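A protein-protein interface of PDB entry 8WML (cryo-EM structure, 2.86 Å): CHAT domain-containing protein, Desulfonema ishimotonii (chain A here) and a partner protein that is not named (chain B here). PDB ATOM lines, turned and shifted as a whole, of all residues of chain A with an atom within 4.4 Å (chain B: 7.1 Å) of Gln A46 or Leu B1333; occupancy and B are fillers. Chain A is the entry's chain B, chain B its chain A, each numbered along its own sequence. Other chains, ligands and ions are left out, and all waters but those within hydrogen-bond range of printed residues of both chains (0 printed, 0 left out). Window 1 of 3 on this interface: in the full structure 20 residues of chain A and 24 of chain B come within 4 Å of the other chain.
The backbone carbonyl oxygen (O) of His B1337 is in hydrogen-bond range of the backbone NH (N) of Gly A47 (3.0 Å).
The backbone carbonyl oxygen (O) of Leu B1333 sits at hydrogen-bond distance from the backbone NH (N) of Leu A48 (3.1 Å).
OE1 of Glu B878 lies close to OE1 of Gln A46, at 2.8 Å.
The backbone carbonyl oxygen (O) of Pro B1338 sits close to the side-chain amide oxygen (OE1) of Gln A46, at 2.7 Å.
Of the 16 printed residues of chain B, 8 touch a printed residue of chain A.
Printed residues of chain B within 4 Å of Arg A4: Lys B879.
Printed residues of chain B within 4 Å of Leu A48: Leu B1333 and Pro B1338.
Leu B1333 touches just these residues of chain A: Tyr A31, Gln A46, Gly A47 and Leu A48.
Leu B1334 touches none of the printed residues of chain A.
Printed residues of chain A within 4 Å of Arg B1336: Gln A45 (3.7 Å), Gln A46 (3.4 Å) and Gly A47 (3.7 Å).
The nearest residue of chain B that does not touch Gln A46 is Gly B1340 (4.2 Å).
The nearest residue of chain A that does not touch Leu B1333 is Ile A3 (4.3 Å).
SG of Cys A44 touches CE of Lys B879, 3.7 Å away.
Glu B878 touches Gln A45.
CE1 of His B1313 touches O of Gln A45, at 3.3 Å.
Arg B1336 touches Gln A45 (NH1 to OE1, 3.7 Å).
CD2 of Leu B1333 touches O of Gln A46, 3.7 Å away.
Arg B1336 touches Gln A46 (CD to O, 3.4 Å).
Gln A46 touches His B1337 (CA to O, 3.3 Å).
Gly A47 touches Leu B1333 (CA to O, 3.2 Å).
Gly A47 touches Arg B1336.
Leu A48 touches Pro B1338.
The side-chain amide nitrogen (ND2) of Asn A1 sits at hydrogen-bond distance from the side-chain sulfur (SG) of Cys A44, 3.2 Å away.
The backbone NH (N) of Arg A4 sits at hydrogen-bond distance from the side-chain amide oxygen (OD1) of Asn A1, 2.9 Å away.
A ring nitrogen (ND1) of His B1337 sits close to the backbone NH (N) of Lys B1339 (3.3 Å).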
ATOM      1  N   ASN A   1       7.630  10.172 -26.781  1.00  0.00           N
ATOM      2  CA  ASN A   1       9.056   9.987 -26.398  1.00  0.00           C
ATOM      3  C   ASN A   1       9.289  10.582 -24.996  1.00  0.00           C
ATOM      4  O   ASN A   1       9.351  11.828 -24.921  1.00  0.00           O
ATOM      5  CB  ASN A   1      10.006  10.583 -27.443  1.00  0.00           C
ATOM      6  CG  ASN A   1      11.453  10.623 -26.998  1.00  0.00           C
ATOM      7  OD1 ASN A   1      11.904  11.603 -26.423  1.00  0.00           O
ATOM      8  ND2 ASN A   1      12.200   9.569 -27.268  1.00  0.00           N
ATOM      9  N   ILE A   3      12.047  10.357 -23.319  1.00  0.00           N
ATOM     10  CA  ILE A   3      13.482  10.552 -23.131  1.00  0.00           C
ATOM     11  C   ILE A   3      13.837  12.033 -23.192  1.00  0.00           C
ATOM     12  O   ILE A   3      14.637  12.526 -22.388  1.00  0.00           O
ATOM     13  CB  ILE A   3      14.273   9.730 -24.169  1.00  0.00           C
ATOM     14  CG1 ILE A   3      14.134   8.229 -23.892  1.00  0.00           C
ATOM     15  CG2 ILE A   3      15.751  10.109 -24.155  1.00  0.00           C
ATOM     16  CD1 ILE A   3      14.197   7.372 -25.133  1.00  0.00           C
ATOM     17  N   ARG A   4      13.252  12.766 -24.144  1.00  0.00           N
ATOM     18  CA  ARG A   4      13.542  14.193 -24.250  1.00  0.00           C
ATOM     19  C   ARG A   4      13.078  14.946 -23.007  1.00  0.00           C
ATOM     20  O   ARG A   4      13.782  15.831 -22.505  1.00  0.00           O
ATOM     21  CB  ARG A   4      12.887  14.781 -25.502  1.00  0.00           C
ATOM     22  CG  ARG A   4      13.488  14.296 -26.818  1.00  0.00           C
ATOM     23  CD  ARG A   4      12.938  15.083 -28.009  1.00  0.00           C
ATOM     24  NE  ARG A   4      11.503  14.913 -28.217  1.00  0.00           N
ATOM     25  CZ  ARG A   4      10.935  13.961 -28.951  1.00  0.00           C
ATOM     26  NH1 ARG A   4      11.651  13.048 -29.592  1.00  0.00           N
ATOM     27  NH2 ARG A   4       9.609  13.924 -29.048  1.00  0.00           N
ATOM     28  N   TYR A  31       8.202   6.762 -18.073  1.00  0.00           N
ATOM     29  CA  TYR A  31       9.094   5.996 -18.939  1.00  0.00           C
ATOM     30  C   TYR A  31       9.052   4.511 -18.600  1.00  0.00           C
ATOM     31  O   TYR A  31       8.998   3.660 -19.498  1.00  0.00           O
ATOM     32  CB  TYR A  31      10.521   6.524 -18.825  1.00  0.00           C
ATOM     33  CG  TYR A  31      11.530   5.720 -19.611  1.00  0.00           C
ATOM     34  CD1 TYR A  31      11.465   5.646 -20.996  1.00  0.00           C
ATOM     35  CD2 TYR A  31      12.541   5.023 -18.965  1.00  0.00           C
ATOM     36  CE1 TYR A  31      12.383   4.907 -21.715  1.00  0.00           C
ATOM     37  CE2 TYR A  31      13.463   4.281 -19.677  1.00  0.00           C
ATOM     38  CZ  TYR A  31      13.379   4.226 -21.049  1.00  0.00           C
ATOM     39  OH  TYR A  31      14.298   3.488 -21.757  1.00  0.00           O
ATOM     40  N   CYS A  44      12.068   4.476 -29.784  1.00  0.00           N
ATOM     41  CA  CYS A  44      13.032   5.543 -29.531  1.00  0.00           C
ATOM     42  C   CYS A  44      14.319   4.922 -29.002  1.00  0.00           C
ATOM     43  O   CYS A  44      14.365   4.456 -27.858  1.00  0.00           O
ATOM     44  CB  CYS A  44      12.458   6.549 -28.540  1.00  0.00           C
ATOM     45  SG  CYS A  44      10.906   7.302 -29.072  1.00  0.00           S
ATOM     46  N   GLN A  45      15.369   4.930 -29.825  1.00  0.00           N
ATOM     47  CA  GLN A  45      16.601   4.193 -29.561  1.00  0.00           C
ATOM     48  C   GLN A  45      17.769   5.112 -29.202  1.00  0.00           C
ATOM     49  O   GLN A  45      18.920   4.793 -29.505  1.00  0.00           O
ATOM     50  CB  GLN A  45      16.971   3.336 -30.773  1.00  0.00           C
ATOM     51  CG  GLN A  45      15.916   2.316 -31.202  1.00  0.00           C
ATOM     52  CD  GLN A  45      15.946   1.049 -30.372  1.00  0.00           C
ATOM     53  OE1 GLN A  45      16.365   1.061 -29.217  1.00  0.00           O
ATOM     54  NE2 GLN A  45      15.506  -0.055 -30.963  1.00  0.00           N
ATOM     55  N   GLN A  46      17.495   6.246 -28.555  1.00  0.00           N
ATOM     56  CA  GLN A  46      18.518   7.217 -28.195  1.00  0.00           C
ATOM     57  C   GLN A  46      18.827   7.137 -26.701  1.00  0.00           C
ATOM     58  O   GLN A  46      18.259   6.331 -25.961  1.00  0.00           O
ATOM     59  CB  GLN A  46      18.081   8.633 -28.579  1.00  0.00           C
ATOM     60  CG  GLN A  46      16.854   9.157 -27.848  1.00  0.00           C
ATOM     61  CD  GLN A  46      16.447  10.532 -28.322  1.00  0.00           C
ATOM     62  OE1 GLN A  46      17.117  11.136 -29.158  1.00  0.00           O
ATOM     63  NE2 GLN A  46      15.342  11.037 -27.792  1.00  0.00           N
ATOM     64  N   GLY A  47      19.745   7.996 -26.262  1.00  0.00           N
ATOM     65  CA  GLY A  47      20.112   8.111 -24.863  1.00  0.00           C
ATOM     66  C   GLY A  47      20.259   9.556 -24.434  1.00  0.00           C
ATOM     67  O   GLY A  47      19.901  10.468 -25.183  1.00  0.00           O
ATOM     68  N   LEU A  48      20.785   9.777 -23.234  1.00  0.00           N
ATOM     69  CA  LEU A  48      20.944  11.115 -22.687  1.00  0.00           C
ATOM     70  C   LEU A  48      22.284  11.721 -23.095  1.00  0.00           C
ATOM     71  O   LEU A  48      23.216  11.021 -23.500  1.00  0.00           O
ATOM     72  CB  LEU A  48      20.832  11.085 -21.162  1.00  0.00           C
ATOM     73  CG  LEU A  48      19.700  10.239 -20.576  1.00  0.00           C
ATOM     74  CD1 LEU A  48      19.626  10.429 -19.071  1.00  0.00           C
ATOM     75  CD2 LEU A  48      18.368  10.584 -21.223  1.00  0.00           C
ATOM     76  N   GLU B 878      16.349   9.130 -35.632  1.00  0.00           N
ATOM     77  CA  GLU B 878      15.839   8.862 -34.293  1.00  0.00           C
ATOM     78  C   GLU B 878      14.786   7.759 -34.276  1.00  0.00           C
ATOM     79  O   GLU B 878      14.668   7.045 -33.275  1.00  0.00           O
ATOM     80  CB  GLU B 878      15.262  10.153 -33.702  1.00  0.00           C
ATOM     81  CG  GLU B 878      14.659  10.019 -32.312  1.00  0.00           C
ATOM     82  CD  GLU B 878      15.641   9.457 -31.315  1.00  0.00           C
ATOM     83  OE1 GLU B 878      16.854   9.686 -31.501  1.00  0.00           O
ATOM     84  OE2 GLU B 878      15.208   8.776 -30.363  1.00  0.00           O
ATOM     85  N   LYS B 879      14.020   7.606 -35.360  1.00  0.00           N
ATOM     86  CA  LYS B 879      12.890   6.678 -35.434  1.00  0.00           C
ATOM     87  C   LYS B 879      13.153   5.653 -36.530  1.00  0.00           C
ATOM     88  O   LYS B 879      12.856   5.910 -37.707  1.00  0.00           O
ATOM     89  CB  LYS B 879      11.588   7.427 -35.715  1.00  0.00           C
ATOM     90  CG  LYS B 879      11.181   8.457 -34.668  1.00  0.00           C
ATOM     91  CD  LYS B 879      10.840   7.819 -33.331  1.00  0.00           C
ATOM     92  CE  LYS B 879      10.258   8.839 -32.366  1.00  0.00           C
ATOM     93  NZ  LYS B 879      11.262   9.841 -31.917  1.00  0.00           N
ATOM     94  N   HIS B1313      25.427   1.941 -29.550  1.00  0.00           N
ATOM     95  CA  HIS B1313      25.201   1.276 -28.267  1.00  0.00           C
ATOM     96  C   HIS B1313      26.512   0.605 -27.870  1.00  0.00           C
ATOM     97  O   HIS B1313      26.820  -0.494 -28.341  1.00  0.00           O
ATOM     98  CB  HIS B1313      24.061   0.266 -28.358  1.00  0.00           C
ATOM     99  CG  HIS B1313      22.740   0.869 -28.725  1.00  0.00           C
ATOM    100  ND1 HIS B1313      22.506   2.227 -28.701  1.00  0.00           N
ATOM    101  CD2 HIS B1313      21.577   0.295 -29.113  1.00  0.00           C
ATOM    102  CE1 HIS B1313      21.260   2.464 -29.065  1.00  0.00           C
ATOM    103  NE2 HIS B1313      20.673   1.309 -29.321  1.00  0.00           N
ATOM    104  N   PRO B1329      15.725   0.943 -14.573  1.00  0.00           N
ATOM    105  CA  PRO B1329      15.488   1.052 -16.021  1.00  0.00           C
ATOM    106  C   PRO B1329      16.378   2.062 -16.728  1.00  0.00           C
ATOM    107  O   PRO B1329      16.854   1.805 -17.837  1.00  0.00           O
ATOM    108  CB  PRO B1329      14.024   1.500 -16.108  1.00  0.00           C
ATOM    109  CG  PRO B1329      13.418   1.128 -14.847  1.00  0.00           C
ATOM    110  CD  PRO B1329      14.479   1.151 -13.811  1.00  0.00           C
ATOM    111  N   GLU B1330      16.609   3.213 -16.098  1.00  0.00           N
ATOM    112  CA  GLU B1330      17.232   4.340 -16.783  1.00  0.00           C
ATOM    113  C   GLU B1330      18.724   4.151 -17.029  1.00  0.00           C
ATOM    114  O   GLU B1330      19.327   4.991 -17.704  1.00  0.00           O
ATOM    115  CB  GLU B1330      16.978   5.642 -16.003  1.00  0.00           C
ATOM    116  CG  GLU B1330      17.761   5.861 -14.690  1.00  0.00           C
ATOM    117  CD  GLU B1330      17.206   5.076 -13.517  1.00  0.00           C
ATOM    118  OE1 GLU B1330      16.221   4.330 -13.703  1.00  0.00           O
ATOM    119  OE2 GLU B1330      17.752   5.211 -12.402  1.00  0.00           O
ATOM    120  N   LYS B1331      19.333   3.086 -16.504  1.00  0.00           N
ATOM    121  CA  LYS B1331      20.757   2.874 -16.730  1.00  0.00           C
ATOM    122  C   LYS B1331      21.070   2.638 -18.202  1.00  0.00           C
ATOM    123  O   LYS B1331      22.156   3.000 -18.666  1.00  0.00           O
ATOM    124  CB  LYS B1331      21.243   1.693 -15.891  1.00  0.00           C
ATOM    125  CG  LYS B1331      22.754   1.530 -15.848  1.00  0.00           C
ATOM    126  CD  LYS B1331      23.135   0.271 -15.094  1.00  0.00           C
ATOM    127  CE  LYS B1331      23.408  -0.896 -16.028  1.00  0.00           C
ATOM    128  NZ  LYS B1331      24.824  -0.921 -16.480  1.00  0.00           N
ATOM    129  N   ARG B1332      20.146   2.034 -18.952  1.00  0.00           N
ATOM    130  CA  ARG B1332      20.412   1.743 -20.356  1.00  0.00           C
ATOM    131  C   ARG B1332      20.526   3.003 -21.203  1.00  0.00           C
ATOM    132  O   ARG B1332      21.160   2.962 -22.262  1.00  0.00           O
ATOM    133  CB  ARG B1332      19.321   0.836 -20.930  1.00  0.00           C
ATOM    134  CG  ARG B1332      17.950   1.484 -21.057  1.00  0.00           C
ATOM    135  CD  ARG B1332      16.896   0.457 -21.422  1.00  0.00           C
ATOM    136  NE  ARG B1332      16.338  -0.200 -20.245  1.00  0.00           N
ATOM    137  CZ  ARG B1332      15.739  -1.385 -20.242  1.00  0.00           C
ATOM    138  NH1 ARG B1332      15.592  -2.097 -21.349  1.00  0.00           N
ATOM    139  NH2 ARG B1332      15.273  -1.870 -19.096  1.00  0.00           N
ATOM    140  N   LEU B1333      19.925   4.113 -20.773  1.00  0.00           N
ATOM    141  CA  LEU B1333      20.001   5.349 -21.542  1.00  0.00           C
ATOM    142  C   LEU B1333      21.370   6.010 -21.469  1.00  0.00           C
ATOM    143  O   LEU B1333      21.640   6.912 -22.269  1.00  0.00           O
ATOM    144  CB  LEU B1333      18.935   6.336 -21.060  1.00  0.00           C
ATOM    145  CG  LEU B1333      17.478   5.869 -21.110  1.00  0.00           C
ATOM    146  CD1 LEU B1333      16.563   6.961 -20.585  1.00  0.00           C
ATOM    147  CD2 LEU B1333      17.069   5.463 -22.519  1.00  0.00           C
ATOM    148  N   LEU B1334      22.233   5.593 -20.544  1.00  0.00           N
ATOM    149  CA  LEU B1334      23.580   6.138 -20.441  1.00  0.00           C
ATOM    150  C   LEU B1334      24.576   5.456 -21.371  1.00  0.00           C
ATOM    151  O   LEU B1334      25.752   5.829 -21.357  1.00  0.00           O
ATOM    152  CB  LEU B1334      24.078   6.030 -18.998  1.00  0.00           C
ATOM    153  CG  LEU B1334      23.334   6.892 -17.977  1.00  0.00           C
ATOM    154  CD1 LEU B1334      23.507   6.330 -16.575  1.00  0.00           C
ATOM    155  CD2 LEU B1334      23.814   8.332 -18.040  1.00  0.00           C
ATOM    156  N   LEU B1335      24.140   4.475 -22.168  1.00  0.00           N
ATOM    157  CA  LEU B1335      25.012   3.742 -23.082  1.00  0.00           C
ATOM    158  C   LEU B1335      24.606   3.898 -24.543  1.00  0.00           C
ATOM    159  O   LEU B1335      25.142   3.181 -25.396  1.00  0.00           O
ATOM    160  CB  LEU B1335      25.033   2.255 -22.711  1.00  0.00           C
ATOM    161  CG  LEU B1335      25.497   1.890 -21.296  1.00  0.00           C
ATOM    162  CD1 LEU B1335      24.834   0.608 -20.832  1.00  0.00           C
ATOM    163  CD2 LEU B1335      27.007   1.754 -21.242  1.00  0.00           C
ATOM    164  N   ARG B1336      23.684   4.812 -24.858  1.00  0.00           N
ATOM    165  CA  ARG B1336      23.197   5.031 -26.212  1.00  0.00           C
ATOM    166  C   ARG B1336      23.507   6.455 -26.656  1.00  0.00           C
ATOM    167  O   ARG B1336      23.594   7.373 -25.835  1.00  0.00           O
ATOM    168  CB  ARG B1336      21.689   4.778 -26.311  1.00  0.00           C
ATOM    169  CG  ARG B1336      21.233   3.468 -25.691  1.00  0.00           C
ATOM    170  CD  ARG B1336      19.756   3.229 -25.928  1.00  0.00           C
ATOM    171  NE  ARG B1336      19.379   1.841 -25.690  1.00  0.00           N
ATOM    172  CZ  ARG B1336      18.130   1.392 -25.641  1.00  0.00           C
ATOM    173  NH1 ARG B1336      17.093   2.196 -25.811  1.00  0.00           N
ATOM    174  NH2 ARG B1336      17.917   0.099 -25.418  1.00  0.00           N
ATOM    175  N   HIS B1337      23.679   6.630 -27.964  1.00  0.00           N
ATOM    176  CA  HIS B1337      23.988   7.946 -28.501  1.00  0.00           C
ATOM    177  C   HIS B1337      22.756   8.848 -28.413  1.00  0.00           C
ATOM    178  O   HIS B1337      21.629   8.370 -28.576  1.00  0.00           O
ATOM    179  CB  HIS B1337      24.449   7.840 -29.953  1.00  0.00           C
ATOM    180  CG  HIS B1337      25.288   8.994 -30.407  1.00  0.00           C
ATOM    181  ND1 HIS B1337      24.780  10.038 -31.149  1.00  0.00           N
ATOM    182  CD2 HIS B1337      26.601   9.269 -30.224  1.00  0.00           C
ATOM    183  CE1 HIS B1337      25.742  10.906 -31.402  1.00  0.00           C
ATOM    184  NE2 HIS B1337      26.857  10.463 -30.853  1.00  0.00           N
ATOM    185  N   PRO B1338      22.923  10.156 -28.160  1.00  0.00           N
ATOM    186  CA  PRO B1338      21.737  11.028 -28.094  1.00  0.00           C
ATOM    187  C   PRO B1338      20.995  11.179 -29.410  1.00  0.00           C
ATOM    188  O   PRO B1338      19.810  11.532 -29.385  1.00  0.00           O
ATOM    189  CB  PRO B1338      22.310  12.376 -27.634  1.00  0.00           C
ATOM    190  CG  PRO B1338      23.640  12.075 -27.082  1.00  0.00           C
ATOM    191  CD  PRO B1338      24.149  10.918 -27.858  1.00  0.00           C
ATOM    192  N   LYS B1339      21.639  10.930 -30.551  1.00  0.00           N
ATOM    193  CA  LYS B1339      21.080  11.253 -31.859  1.00  0.00           C
ATOM    194  C   LYS B1339      20.506  10.046 -32.596  1.00  0.00           C
ATOM    195  O   LYS B1339      20.105  10.186 -33.755  1.00  0.00           O
ATOM    196  CB  LYS B1339      22.145  11.925 -32.727  1.00  0.00           C
ATOM    197  CG  LYS B1339      22.577  13.292 -32.226  1.00  0.00           C
ATOM    198  CD  LYS B1339      23.610  13.920 -33.148  1.00  0.00           C
ATOM    199  CE  LYS B1339      23.994  15.319 -32.688  1.00  0.00           C
ATOM    200  NZ  LYS B1339      24.727  15.304 -31.392  1.00  0.00           N
ATOM    201  N   GLY B1340      20.469   8.870 -31.970  1.00  0.00           N
ATOM    202  CA  GLY B1340      19.823   7.710 -32.560  1.00  0.00           C
ATOM    203  C   GLY B1340      20.767   6.669 -33.126  1.00  0.00           C
ATOM    204  O   GLY B1340      21.773   6.329 -32.497  1.00  0.00           O
ATOM    205  N   LEU B1341      20.446   6.155 -34.314  1.00  0.00           N
ATOM    206  CA  LEU B1341      21.152   5.041 -34.932  1.00  0.00           C
ATOM    207  C   LEU B1341      21.668   5.436 -36.308  1.00  0.00           C
ATOM    208  O   LEU B1341      20.985   6.137 -37.062  1.00  0.00           O
ATOM    209  CB  LEU B1341      20.240   3.817 -35.066  1.00  0.00           C
ATOM    210  CG  LEU B1341      19.801   3.122 -33.777  1.00  0.00           C
ATOM    211  CD1 LEU B1341      18.761   2.065 -34.088  1.00  0.00           C
ATOM    212  CD2 LEU B1341      20.983   2.501 -33.052  1.00  0.00           C
